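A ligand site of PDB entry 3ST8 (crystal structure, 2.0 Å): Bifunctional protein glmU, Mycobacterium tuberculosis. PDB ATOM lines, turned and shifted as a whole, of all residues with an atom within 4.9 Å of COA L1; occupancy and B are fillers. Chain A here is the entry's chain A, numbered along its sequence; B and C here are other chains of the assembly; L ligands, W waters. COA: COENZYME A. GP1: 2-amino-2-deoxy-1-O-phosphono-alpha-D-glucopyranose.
The backbone NH (N) of Ser 422 is in hydrogen-bond range of an oxygen (O5P) of COA L1 (2.7 Å). The side-chain hydroxyl (OG) of Ser 422 lies close to an oxygen (O5P) of COA L1 (3.3 Å). O5A of COA L1 lies within salt-bridge range of NZ of Lys 470 of chain B, at 2.9 Å. O9P of COA L1 lies within hydrogen-bond range of N of Ala 440 (2.9 Å). The backbone carbonyl oxygen (O) of Ala 440 lies within hydrogen-bond range of a nitrogen (N6A) of COA L1, at 2.9 Å. O of Tyr 404 of chain C is in hydrogen-bond range of N4P of COA L1, at 3.0 Å. An oxygen (O8A) of COA L1 is in salt-bridge range of the guanidinium group (NH2) of Arg 461 of chain B, at 3.1 Å. The indole nitrogen of Trp 466 of chain B sits at hydrogen-bond distance from an oxygen (O2A) of COA L1, 3.0 Å away. S1P of COA L1 sits close to N of Ala 397, 3.2 Å away. A nitrogen (N2) of GP1 L2 lies within hydrogen-bond range of a ring nitrogen (NE2) of His 380, at 3.2 Å. N2 of GP1 L2 lies within hydrogen-bond range of OD1 of Asn 403 of chain C, at 2.9 Å. The side-chain amide oxygen (OD1) of Asn 394 sits at hydrogen-bond distance from an oxygen (O4) of GP1 L2, 2.6 Å away.
A sulfur (S1P) of COA L1 sits close to an oxygen (O3) of GP1 L2 (3.0 Å).
O of Val 455 is in hydrogen-bond range of N of Arg 461 of chain B (2.8 Å). The backbone NH of Gly 421 lies within hydrogen-bond range of the side-chain hydroxyl of Thr 438 (2.6 Å). O of Val 443 of chain C is in hydrogen-bond range of NH2 of Arg 445 of chain C (2.9 Å). The backbone NH (N) of Ile 463 of chain B is in hydrogen-bond range of the backbone carbonyl oxygen (O) of Leu 453 (2.8 Å). The guanidinium group (NH2) of Arg 471 of chain B is in hydrogen-bond range of the backbone carbonyl oxygen (O) of Asp 405 of chain C, at 2.9 Å. N of Gly 396 is in hydrogen-bond range of O of Thr 420 (3.0 Å).
Gly 396 touches COA L1 (CA to C3P, 3.8 Å). CA of Gly 421 touches O5P of COA L1, at 3.2 Å. Gly 439 touches COA L1. Leu 453 touches COA L1. Val 455 touches COA L1. O of Ala 457 touches C2A of COA L1, at 3.3 Å. CD1 of Ile 463 of chain B touches C4B of COA L1, at 3.6 Å. Arg 471 of chain B touches COA L1. CG1 of Val 402 of chain C touches C5P of COA L1 (3.2 Å). CG1 of Val 427 of chain C touches N8P of COA L1, 3.8 Å away. Val 443 of chain C touches COA L1. Arg 445 of chain C touches COA L1. Hydrophobic or aromatic side chains within 4 Å of COA L1: Ala 397, Leu 453, Val 455, Ala 457, Ile 463 of chain B, Trp 466 of chain B, Val 402 of chain C, Val 427 of chain C and Val 443 of chain C. Along chain A the residues within 4 Å of COA L1 span positions 396 to 457. The nearest printed residue that does not touch COA L1 is His 380 (4.2 Å).
Water W7 lies within hydrogen-bond range of a nitrogen (N1A) of COA L1 (2.8 Å), the backbone NH of Ala 457 (2.8 Å), the backbone NH of Ser 456 (2.8 Å) and the backbone carbonyl oxygen of Ala 440 (3.2 Å). Water W5 bridges O4A of COA L1 and NH2 of Arg 471 of chain B. Water W4 lies within hydrogen-bond range of the guanidinium group of Arg 461 of chain B (2.9 Å) and a nitrogen (N3A) of COA L1 (3.0 Å). Water W1 bridges N4P of COA L1 (3.1 Å) and O of Tyr 404 of chain C (3.5 Å). Water W2 lies within hydrogen-bond range of O of Ala 457, NH1 of Arg 445 of chain C and N3A of COA L1.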
ATOM      1  N   HIS A 380      35.086  -6.015 -35.715  1.00  0.00           N
ATOM      2  CA  HIS A 380      35.749  -4.730 -35.291  1.00  0.00           C
ATOM      3  C   HIS A 380      36.152  -4.732 -33.847  1.00  0.00           C
ATOM      4  O   HIS A 380      35.323  -4.936 -32.944  1.00  0.00           O
ATOM      5  CB  HIS A 380      34.730  -3.499 -35.360  1.00  0.00           C
ATOM      6  CG  HIS A 380      33.810  -3.487 -36.603  1.00  0.00           C
ATOM      7  ND1 HIS A 380      34.261  -3.085 -37.853  1.00  0.00           N
ATOM      8  CD2 HIS A 380      32.480  -3.726 -36.736  1.00  0.00           C
ATOM      9  CE1 HIS A 380      33.249  -3.119 -38.709  1.00  0.00           C
ATOM     10  NE2 HIS A 380      32.156  -3.478 -38.043  1.00  0.00           N
ATOM     11  N   ASN A 394      27.354 -13.190 -35.422  1.00  0.00           N
ATOM     12  CA  ASN A 394      28.025 -11.908 -35.611  1.00  0.00           C
ATOM     13  C   ASN A 394      28.314 -11.359 -34.207  1.00  0.00           C
ATOM     14  O   ASN A 394      27.428 -11.355 -33.317  1.00  0.00           O
ATOM     15  CB  ASN A 394      27.045 -10.905 -36.262  1.00  0.00           C
ATOM     16  CG  ASN A 394      27.765  -9.649 -36.756  1.00  0.00           C
ATOM     17  OD1 ASN A 394      28.517  -9.745 -37.773  1.00  0.00           O
ATOM     18  ND2 ASN A 394      27.655  -8.518 -36.040  1.00  0.00           N
ATOM     19  N   GLY A 396      29.390  -8.127 -32.080  1.00  0.00           N
ATOM     20  CA  GLY A 396      29.321  -6.705 -32.351  1.00  0.00           C
ATOM     21  C   GLY A 396      30.643  -6.034 -32.033  1.00  0.00           C
ATOM     22  O   GLY A 396      31.474  -6.585 -31.299  1.00  0.00           O
ATOM     23  N   ALA A 397      30.826  -4.852 -32.628  1.00  0.00           N
ATOM     24  CA  ALA A 397      32.084  -4.104 -32.515  1.00  0.00           C
ATOM     25  C   ALA A 397      32.442  -3.871 -31.072  1.00  0.00           C
ATOM     26  O   ALA A 397      31.590  -3.619 -30.247  1.00  0.00           O
ATOM     27  CB  ALA A 397      31.917  -2.742 -33.163  1.00  0.00           C
ATOM     28  N   THR A 420      25.372 -10.660 -31.285  1.00  0.00           N
ATOM     29  CA  THR A 420      25.604  -9.972 -30.007  1.00  0.00           C
ATOM     30  C   THR A 420      25.889  -8.480 -30.263  1.00  0.00           C
ATOM     31  O   THR A 420      26.475  -8.091 -31.282  1.00  0.00           O
ATOM     32  CB  THR A 420      26.809 -10.657 -29.213  1.00  0.00           C
ATOM     33  OG1 THR A 420      27.943 -10.675 -30.063  1.00  0.00           O
ATOM     34  CG2 THR A 420      26.477 -12.122 -28.922  1.00  0.00           C
ATOM     35  N   GLY A 421      25.579  -7.677 -29.297  1.00  0.00           N
ATOM     36  CA  GLY A 421      25.623  -6.221 -29.534  1.00  0.00           C
ATOM     37  C   GLY A 421      27.009  -5.670 -29.358  1.00  0.00           C
ATOM     38  O   GLY A 421      27.874  -6.315 -28.667  1.00  0.00           O
ATOM     39  N   SER A 422      27.256  -4.499 -29.970  1.00  0.00           N
ATOM     40  CA  SER A 422      28.508  -3.806 -29.720  1.00  0.00           C
ATOM     41  C   SER A 422      28.764  -3.560 -28.213  1.00  0.00           C
ATOM     42  O   SER A 422      27.835  -3.379 -27.438  1.00  0.00           O
ATOM     43  CB  SER A 422      28.494  -2.372 -30.371  1.00  0.00           C
ATOM     44  OG  SER A 422      28.149  -2.554 -31.743  1.00  0.00           O
ATOM     45  N   THR A 438      22.444  -9.823 -27.892  1.00  0.00           N
ATOM     46  CA  THR A 438      22.620  -9.005 -26.663  1.00  0.00           C
ATOM     47  C   THR A 438      22.488  -7.567 -27.144  1.00  0.00           C
ATOM     48  O   THR A 438      22.808  -7.272 -28.301  1.00  0.00           O
ATOM     49  CB  THR A 438      24.049  -9.144 -26.010  1.00  0.00           C
ATOM     50  OG1 THR A 438      25.065  -8.702 -26.910  1.00  0.00           O
ATOM     51  CG2 THR A 438      24.378 -10.663 -25.706  1.00  0.00           C
ATOM     52  N   GLY A 439      22.123  -6.662 -26.250  1.00  0.00           N
ATOM     53  CA  GLY A 439      22.041  -5.250 -26.688  1.00  0.00           C
ATOM     54  C   GLY A 439      23.393  -4.631 -26.679  1.00  0.00           C
ATOM     55  O   GLY A 439      24.352  -5.147 -26.031  1.00  0.00           O
ATOM     56  N   ALA A 440      23.548  -3.513 -27.390  1.00  0.00           N
ATOM     57  CA  ALA A 440      24.824  -2.732 -27.229  1.00  0.00           C
ATOM     58  C   ALA A 440      25.055  -2.366 -25.733  1.00  0.00           C
ATOM     59  O   ALA A 440      24.107  -2.076 -24.991  1.00  0.00           O
ATOM     60  CB  ALA A 440      24.757  -1.422 -28.045  1.00  0.00           C
ATOM     61  N   LEU A 453      17.008 -12.025 -25.620  1.00  0.00           N
ATOM     62  CA  LEU A 453      17.842 -10.806 -25.723  1.00  0.00           C
ATOM     63  C   LEU A 453      18.409 -10.527 -24.337  1.00  0.00           C
ATOM     64  O   LEU A 453      17.627 -10.410 -23.355  1.00  0.00           O
ATOM     65  CB  LEU A 453      16.993  -9.598 -26.157  1.00  0.00           C
ATOM     66  CG  LEU A 453      17.611  -8.169 -25.922  1.00  0.00           C
ATOM     67  CD1 LEU A 453      18.772  -7.978 -26.856  1.00  0.00           C
ATOM     68  CD2 LEU A 453      16.576  -7.105 -26.294  1.00  0.00           C
ATOM     69  N   VAL A 455      20.372  -7.838 -21.898  1.00  0.00           N
ATOM     70  CA  VAL A 455      20.761  -6.414 -21.846  1.00  0.00           C
ATOM     71  C   VAL A 455      21.149  -6.137 -20.390  1.00  0.00           C
ATOM     72  O   VAL A 455      20.882  -6.963 -19.445  1.00  0.00           O
ATOM     73  CB  VAL A 455      19.588  -5.399 -22.263  1.00  0.00           C
ATOM     74  CG1 VAL A 455      19.198  -5.557 -23.765  1.00  0.00           C
ATOM     75  CG2 VAL A 455      18.297  -5.632 -21.365  1.00  0.00           C
ATOM     76  N   SER A 456      21.848  -5.020 -20.179  1.00  0.00           N
ATOM     77  CA  SER A 456      22.153  -4.622 -18.831  1.00  0.00           C
ATOM     78  C   SER A 456      22.348  -3.129 -18.674  1.00  0.00           C
ATOM     79  O   SER A 456      22.210  -2.633 -17.567  1.00  0.00           O
ATOM     80  CB  SER A 456      23.416  -5.349 -18.300  1.00  0.00           C
ATOM     81  OG  SER A 456      24.545  -4.907 -19.040  1.00  0.00           O
ATOM     82  N   ALA A 457      22.610  -2.369 -19.753  1.00  0.00           N
ATOM     83  CA  ALA A 457      22.773  -0.907 -19.538  1.00  0.00           C
ATOM     84  C   ALA A 457      21.465  -0.245 -18.974  1.00  0.00           C
ATOM     85  O   ALA A 457      20.322  -0.709 -19.263  1.00  0.00           O
ATOM     86  CB  ALA A 457      23.131  -0.248 -20.890  1.00  0.00           C
ATOM     87  N   ARG B 461      19.592  -8.623 -17.656  1.00  0.00           N
ATOM     88  CA  ARG B 461      18.206  -9.010 -17.744  1.00  0.00           C
ATOM     89  C   ARG B 461      18.090  -9.859 -18.992  1.00  0.00           C
ATOM     90  O   ARG B 461      18.495  -9.431 -20.114  1.00  0.00           O
ATOM     91  CB  ARG B 461      17.292  -7.736 -17.835  1.00  0.00           C
ATOM     92  CG  ARG B 461      15.846  -8.186 -17.984  1.00  0.00           C
ATOM     93  CD  ARG B 461      14.822  -7.091 -17.846  1.00  0.00           C
ATOM     94  NE  ARG B 461      15.167  -5.858 -18.551  1.00  0.00           N
ATOM     95  CZ  ARG B 461      14.306  -5.230 -19.358  1.00  0.00           C
ATOM     96  NH1 ARG B 461      13.120  -5.775 -19.580  1.00  0.00           N
ATOM     97  NH2 ARG B 461      14.640  -4.089 -19.958  1.00  0.00           N
ATOM     98  N   ILE B 463      15.603 -11.370 -21.721  1.00  0.00           N
ATOM     99  CA  ILE B 463      14.211 -11.201 -22.167  1.00  0.00           C
ATOM    100  C   ILE B 463      13.974 -12.417 -23.042  1.00  0.00           C
ATOM    101  O   ILE B 463      14.433 -12.467 -24.214  1.00  0.00           O
ATOM    102  CB  ILE B 463      14.012  -9.890 -22.938  1.00  0.00           C
ATOM    103  CG1 ILE B 463      14.450  -8.702 -22.000  1.00  0.00           C
ATOM    104  CG2 ILE B 463      12.407  -9.793 -23.452  1.00  0.00           C
ATOM    105  CD1 ILE B 463      14.496  -7.383 -22.735  1.00  0.00           C
ATOM    106  N   TRP B 466      12.575 -12.975 -27.041  1.00  0.00           N
ATOM    107  CA  TRP B 466      12.631 -11.641 -27.752  1.00  0.00           C
ATOM    108  C   TRP B 466      12.864 -11.896 -29.234  1.00  0.00           C
ATOM    109  O   TRP B 466      12.293 -11.255 -30.137  1.00  0.00           O
ATOM    110  CB  TRP B 466      13.754 -10.760 -27.123  1.00  0.00           C
ATOM    111  CG  TRP B 466      13.877  -9.388 -27.747  1.00  0.00           C
ATOM    112  CD1 TRP B 466      13.237  -8.223 -27.378  1.00  0.00           C
ATOM    113  CD2 TRP B 466      14.625  -9.096 -28.919  1.00  0.00           C
ATOM    114  NE1 TRP B 466      13.627  -7.198 -28.221  1.00  0.00           N
ATOM    115  CE2 TRP B 466      14.459  -7.727 -29.189  1.00  0.00           C
ATOM    116  CE3 TRP B 466      15.501  -9.857 -29.735  1.00  0.00           C
ATOM    117  CZ2 TRP B 466      15.113  -7.066 -30.281  1.00  0.00           C
ATOM    118  CZ3 TRP B 466      16.164  -9.195 -30.848  1.00  0.00           C
ATOM    119  CH2 TRP B 466      15.902  -7.796 -31.123  1.00  0.00           C
ATOM    120  N   LYS B 470      10.648 -10.286 -32.087  1.00  0.00           N
ATOM    121  CA  LYS B 470      11.073  -9.027 -32.704  1.00  0.00           C
ATOM    122  C   LYS B 470      11.868  -9.227 -33.964  1.00  0.00           C
ATOM    123  O   LYS B 470      12.102  -8.263 -34.719  1.00  0.00           O
ATOM    124  CB  LYS B 470      11.895  -8.152 -31.673  1.00  0.00           C
ATOM    125  CG  LYS B 470      11.222  -7.782 -30.416  1.00  0.00           C
ATOM    126  CD  LYS B 470       9.816  -7.149 -30.582  1.00  0.00           C
ATOM    127  CE  LYS B 470       9.974  -5.799 -31.256  1.00  0.00           C
ATOM    128  NZ  LYS B 470      10.585  -4.717 -30.321  1.00  0.00           N
ATOM    129  N   ARG B 471      12.340 -10.433 -34.215  1.00  0.00           N
ATOM    130  CA  ARG B 471      13.027 -10.743 -35.494  1.00  0.00           C
ATOM    131  C   ARG B 471      12.328 -11.992 -36.161  1.00  0.00           C
ATOM    132  O   ARG B 471      12.990 -12.953 -36.558  1.00  0.00           O
ATOM    133  CB  ARG B 471      14.553 -11.058 -35.258  1.00  0.00           C
ATOM    134  CG  ARG B 471      15.271  -9.787 -34.723  1.00  0.00           C
ATOM    135  CD  ARG B 471      15.400  -8.686 -35.766  1.00  0.00           C
ATOM    136  NE  ARG B 471      16.225  -7.553 -35.201  1.00  0.00           N
ATOM    137  CZ  ARG B 471      15.725  -6.533 -34.535  1.00  0.00           C
ATOM    138  NH1 ARG B 471      14.419  -6.504 -34.275  1.00  0.00           N
ATOM    139  NH2 ARG B 471      16.516  -5.563 -34.095  1.00  0.00           N
ATOM    140  N   VAL C 400      31.178   3.372 -30.664  1.00  0.00           N
ATOM    141  CA  VAL C 400      30.770   2.597 -31.858  1.00  0.00           C
ATOM    142  C   VAL C 400      29.501   3.272 -32.452  1.00  0.00           C
ATOM    143  O   VAL C 400      28.547   3.500 -31.695  1.00  0.00           O
ATOM    144  CB  VAL C 400      30.399   1.133 -31.521  1.00  0.00           C
ATOM    145  CG1 VAL C 400      29.909   0.395 -32.889  1.00  0.00           C
ATOM    146  CG2 VAL C 400      31.698   0.383 -30.946  1.00  0.00           C
ATOM    147  N   VAL C 402      26.625   2.209 -34.034  1.00  0.00           N
ATOM    148  CA  VAL C 402      26.120   0.851 -34.103  1.00  0.00           C
ATOM    149  C   VAL C 402      25.183   0.909 -35.265  1.00  0.00           C
ATOM    150  O   VAL C 402      24.033   1.371 -35.121  1.00  0.00           O
ATOM    151  CB  VAL C 402      25.388   0.508 -32.786  1.00  0.00           C
ATOM    152  CG1 VAL C 402      24.624  -0.808 -32.851  1.00  0.00           C
ATOM    153  CG2 VAL C 402      26.401   0.505 -31.605  1.00  0.00           C
ATOM    154  N   ASN C 403      25.601   0.424 -36.420  1.00  0.00           N
ATOM    155  CA  ASN C 403      24.781   0.695 -37.594  1.00  0.00           C
ATOM    156  C   ASN C 403      24.027  -0.596 -38.076  1.00  0.00           C
ATOM    157  O   ASN C 403      23.613  -0.618 -39.196  1.00  0.00           O
ATOM    158  CB  ASN C 403      25.700   1.154 -38.728  1.00  0.00           C
ATOM    159  CG  ASN C 403      26.710  -0.002 -39.208  1.00  0.00           C
ATOM    160  OD1 ASN C 403      27.055  -0.931 -38.438  1.00  0.00           O
ATOM    161  ND2 ASN C 403      27.136   0.069 -40.478  1.00  0.00           N
ATOM    162  N   TYR C 404      23.928  -1.656 -37.262  1.00  0.00           N
ATOM    163  CA  TYR C 404      23.384  -2.946 -37.763  1.00  0.00           C
ATOM    164  C   TYR C 404      22.481  -3.460 -36.712  1.00  0.00           C
ATOM    165  O   TYR C 404      22.932  -3.806 -35.568  1.00  0.00           O
ATOM    166  CB  TYR C 404      24.540  -3.965 -37.897  1.00  0.00           C
ATOM    167  CG  TYR C 404      24.209  -5.358 -38.326  1.00  0.00           C
ATOM    168  CD1 TYR C 404      23.473  -5.593 -39.530  1.00  0.00           C
ATOM    169  CD2 TYR C 404      24.746  -6.492 -37.632  1.00  0.00           C
ATOM    170  CE1 TYR C 404      23.236  -6.898 -39.999  1.00  0.00           C
ATOM    171  CE2 TYR C 404      24.502  -7.834 -38.120  1.00  0.00           C
ATOM    172  CZ  TYR C 404      23.738  -8.018 -39.271  1.00  0.00           C
ATOM    173  OH  TYR C 404      23.529  -9.271 -39.790  1.00  0.00           O
ATOM    174  N   ASP C 405      21.201  -3.623 -37.054  1.00  0.00           N
ATOM    175  CA  ASP C 405      20.232  -4.000 -36.002  1.00  0.00           C
ATOM    176  C   ASP C 405      20.086  -5.548 -35.946  1.00  0.00           C
ATOM    177  O   ASP C 405      19.110  -6.073 -35.294  1.00  0.00           O
ATOM    178  CB  ASP C 405      18.856  -3.337 -36.306  1.00  0.00           C
ATOM    179  CG  ASP C 405      18.281  -3.839 -37.615  1.00  0.00           C
ATOM    180  OD1 ASP C 405      17.353  -3.163 -38.109  1.00  0.00           O
ATOM    181  OD2 ASP C 405      18.774  -4.875 -38.226  1.00  0.00           O
ATOM    182  N   VAL C 427      23.114   3.966 -31.090  1.00  0.00           N
ATOM    183  CA  VAL C 427      22.320   2.815 -31.647  1.00  0.00           C
ATOM    184  C   VAL C 427      21.432   3.432 -32.757  1.00  0.00           C
ATOM    185  O   VAL C 427      20.401   4.026 -32.448  1.00  0.00           O
ATOM    186  CB  VAL C 427      21.507   2.053 -30.556  1.00  0.00           C
ATOM    187  CG1 VAL C 427      20.653   0.862 -31.193  1.00  0.00           C
ATOM    188  CG2 VAL C 427      22.455   1.586 -29.426  1.00  0.00           C
ATOM    189  N   VAL C 443      24.898   4.342 -23.627  1.00  0.00           N
ATOM    190  CA  VAL C 443      24.318   3.682 -24.802  1.00  0.00           C
ATOM    191  C   VAL C 443      23.159   4.576 -25.265  1.00  0.00           C
ATOM    192  O   VAL C 443      22.189   4.758 -24.521  1.00  0.00           O
ATOM    193  CB  VAL C 443      23.764   2.291 -24.408  1.00  0.00           C
ATOM    194  CG1 VAL C 443      23.112   1.659 -25.622  1.00  0.00           C
ATOM    195  CG2 VAL C 443      24.964   1.377 -23.851  1.00  0.00           C
ATOM    196  N   ARG C 445      20.186   5.436 -27.313  1.00  0.00           N
ATOM    197  CA  ARG C 445      19.129   4.762 -28.073  1.00  0.00           C
ATOM    198  C   ARG C 445      18.057   5.763 -28.540  1.00  0.00           C
ATOM    199  O   ARG C 445      17.214   5.363 -29.376  1.00  0.00           O
ATOM    200  CB  ARG C 445      18.475   3.616 -27.228  1.00  0.00           C
ATOM    201  CG  ARG C 445      19.390   2.326 -27.088  1.00  0.00           C
ATOM    202  CD  ARG C 445      19.036   1.678 -25.656  1.00  0.00           C
ATOM    203  NE  ARG C 445      19.806   2.559 -24.685  1.00  0.00           N
ATOM    204  CZ  ARG C 445      19.804   2.426 -23.351  1.00  0.00           C
ATOM    205  NH1 ARG C 445      19.021   1.481 -22.782  1.00  0.00           N
ATOM    206  NH2 ARG C 445      20.567   3.243 -22.609  1.00  0.00           N
HETATM  207  N1A COA L   1      20.789  -1.763 -23.393  1.00  0.00           N
HETATM  208  C2A COA L   1      19.920  -1.817 -22.386  1.00  0.00           C
HETATM  209  N3A COA L   1      18.623  -2.008 -22.548  1.00  0.00           N
HETATM  210  C4A COA L   1      18.148  -2.084 -23.806  1.00  0.00           C
HETATM  211  C5A COA L   1      19.004  -2.010 -24.876  1.00  0.00           C
HETATM  212  C6A COA L   1      20.389  -1.865 -24.655  1.00  0.00           C
HETATM  213  N6A COA L   1      21.266  -1.819 -25.698  1.00  0.00           N
HETATM  214  N7A COA L   1      18.264  -2.141 -26.005  1.00  0.00           N
HETATM  215  C8A COA L   1      16.961  -2.374 -25.608  1.00  0.00           C
HETATM  216  N9A COA L   1      16.915  -2.304 -24.272  1.00  0.00           N
HETATM  217  C1B COA L   1      15.738  -2.556 -23.409  1.00  0.00           C
HETATM  218  C2B COA L   1      14.559  -1.695 -23.906  1.00  0.00           C
HETATM  219  O2B COA L   1      14.625  -0.650 -22.934  1.00  0.00           O
HETATM  220  C3B COA L   1      13.364  -2.670 -23.680  1.00  0.00           C
HETATM  221  O3B COA L   1      13.180  -2.786 -22.266  1.00  0.00           O
HETATM  222  P3B COA L   1      11.776  -2.228 -21.528  1.00  0.00           P
HETATM  223  O7A COA L   1      10.768  -3.036 -22.368  1.00  0.00           O
HETATM  224  O8A COA L   1      12.058  -2.329 -19.996  1.00  0.00           O
HETATM  225  O9A COA L   1      11.782  -0.706 -21.740  1.00  0.00           O
HETATM  226  C4B COA L   1      13.881  -4.030 -24.015  1.00  0.00           C
HETATM  227  O4B COA L   1      15.374  -3.891 -23.928  1.00  0.00           O
HETATM  228  C5B COA L   1      13.272  -4.460 -25.355  1.00  0.00           C
HETATM  229  O5B COA L   1      13.947  -3.510 -26.139  1.00  0.00           O
HETATM  230  P1A COA L   1      13.055  -3.044 -27.357  1.00  0.00           P
HETATM  231  O1A COA L   1      11.870  -2.204 -27.221  1.00  0.00           O
HETATM  232  O2A COA L   1      12.493  -4.445 -27.578  1.00  0.00           O
HETATM  233  O3A COA L   1      13.980  -2.264 -28.444  1.00  0.00           O
HETATM  234  P2A COA L   1      14.204  -3.190 -29.708  1.00  0.00           P
HETATM  235  O4A COA L   1      14.046  -2.502 -31.029  1.00  0.00           O
HETATM  236  O5A COA L   1      13.279  -4.341 -29.413  1.00  0.00           O
HETATM  237  O6A COA L   1      15.748  -3.676 -29.629  1.00  0.00           O
HETATM  238  CBP COA L   1      18.069  -3.491 -29.791  1.00  0.00           C
HETATM  239  CCP COA L   1      16.720  -2.715 -29.697  1.00  0.00           C
HETATM  240  CDP COA L   1      18.362  -4.421 -28.654  1.00  0.00           C
HETATM  241  CEP COA L   1      18.144  -4.214 -31.126  1.00  0.00           C
HETATM  242  CAP COA L   1      19.006  -2.303 -29.803  1.00  0.00           C
HETATM  243  OAP COA L   1      18.708  -1.421 -28.649  1.00  0.00           O
HETATM  244  C9P COA L   1      20.486  -2.700 -29.671  1.00  0.00           C
HETATM  245  O9P COA L   1      20.985  -2.748 -28.537  1.00  0.00           O
HETATM  246  N8P COA L   1      21.141  -2.883 -30.833  1.00  0.00           N
HETATM  247  C7P COA L   1      22.562  -3.282 -30.934  1.00  0.00           C
HETATM  248  C6P COA L   1      22.856  -3.775 -32.335  1.00  0.00           C
HETATM  249  C5P COA L   1      24.375  -3.965 -32.379  1.00  0.00           C
HETATM  250  O5P COA L   1      25.093  -3.630 -31.388  1.00  0.00           O
HETATM  251  N4P COA L   1      24.935  -4.444 -33.478  1.00  0.00           N
HETATM  252  C3P COA L   1      26.376  -4.687 -33.726  1.00  0.00           C
HETATM  253  C2P COA L   1      26.964  -3.446 -34.474  1.00  0.00           C
HETATM  254  S1P COA L   1      28.762  -3.771 -34.808  1.00  0.00           S
HETATM  255  C1  GP1 L   2      28.189  -3.824 -39.915  1.00  0.00           C
HETATM  256  C2  GP1 L   2      28.308  -4.165 -38.420  1.00  0.00           C
HETATM  257  C3  GP1 L   2      29.012  -5.551 -38.236  1.00  0.00           C
HETATM  258  C4  GP1 L   2      28.491  -6.666 -39.217  1.00  0.00           C
HETATM  259  C5  GP1 L   2      28.090  -6.210 -40.680  1.00  0.00           C
HETATM  260  C6  GP1 L   2      27.268  -7.271 -41.523  1.00  0.00           C
HETATM  261  N2  GP1 L   2      28.987  -2.963 -37.832  1.00  0.00           N
HETATM  262  O1  GP1 L   2      29.524  -3.652 -40.451  1.00  0.00           O
HETATM  263  O3  GP1 L   2      28.746  -6.005 -36.863  1.00  0.00           O
HETATM  264  O4  GP1 L   2      29.373  -7.769 -39.303  1.00  0.00           O
HETATM  265  O6  GP1 L   2      27.191  -6.759 -42.883  1.00  0.00           O
HETATM  266  O5  GP1 L   2      27.445  -4.861 -40.656  1.00  0.00           O
HETATM  267  O7B GP1 L   2      30.771  -1.689 -41.673  1.00  0.00           O
HETATM  268  P4B GP1 L   2      29.671  -2.818 -41.882  1.00  0.00           P
HETATM  269  O8B GP1 L   2      28.250  -2.273 -42.330  1.00  0.00           O
HETATM  270  O9B GP1 L   2      30.212  -3.760 -42.936  1.00  0.00           O
HETATM  271  O   HOH W   1      23.207  -6.982 -34.164  1.00  0.00           O
HETATM  272  O   HOH W   2      17.813   0.141 -20.177  1.00  0.00           O
HETATM  273  O   HOH W   3      20.097  -1.969 -33.352  1.00  0.00           O
HETATM  274  O   HOH W   4      16.896  -2.333 -20.176  1.00  0.00           O
HETATM  275  O   HOH W   5      15.469  -2.896 -33.389  1.00  0.00           O
HETATM  276  O   HOH W   6      17.157   0.710 -29.000  1.00  0.00           O
HETATM  277  O   HOH W   7      22.749  -3.439 -22.372  1.00  0.00           O
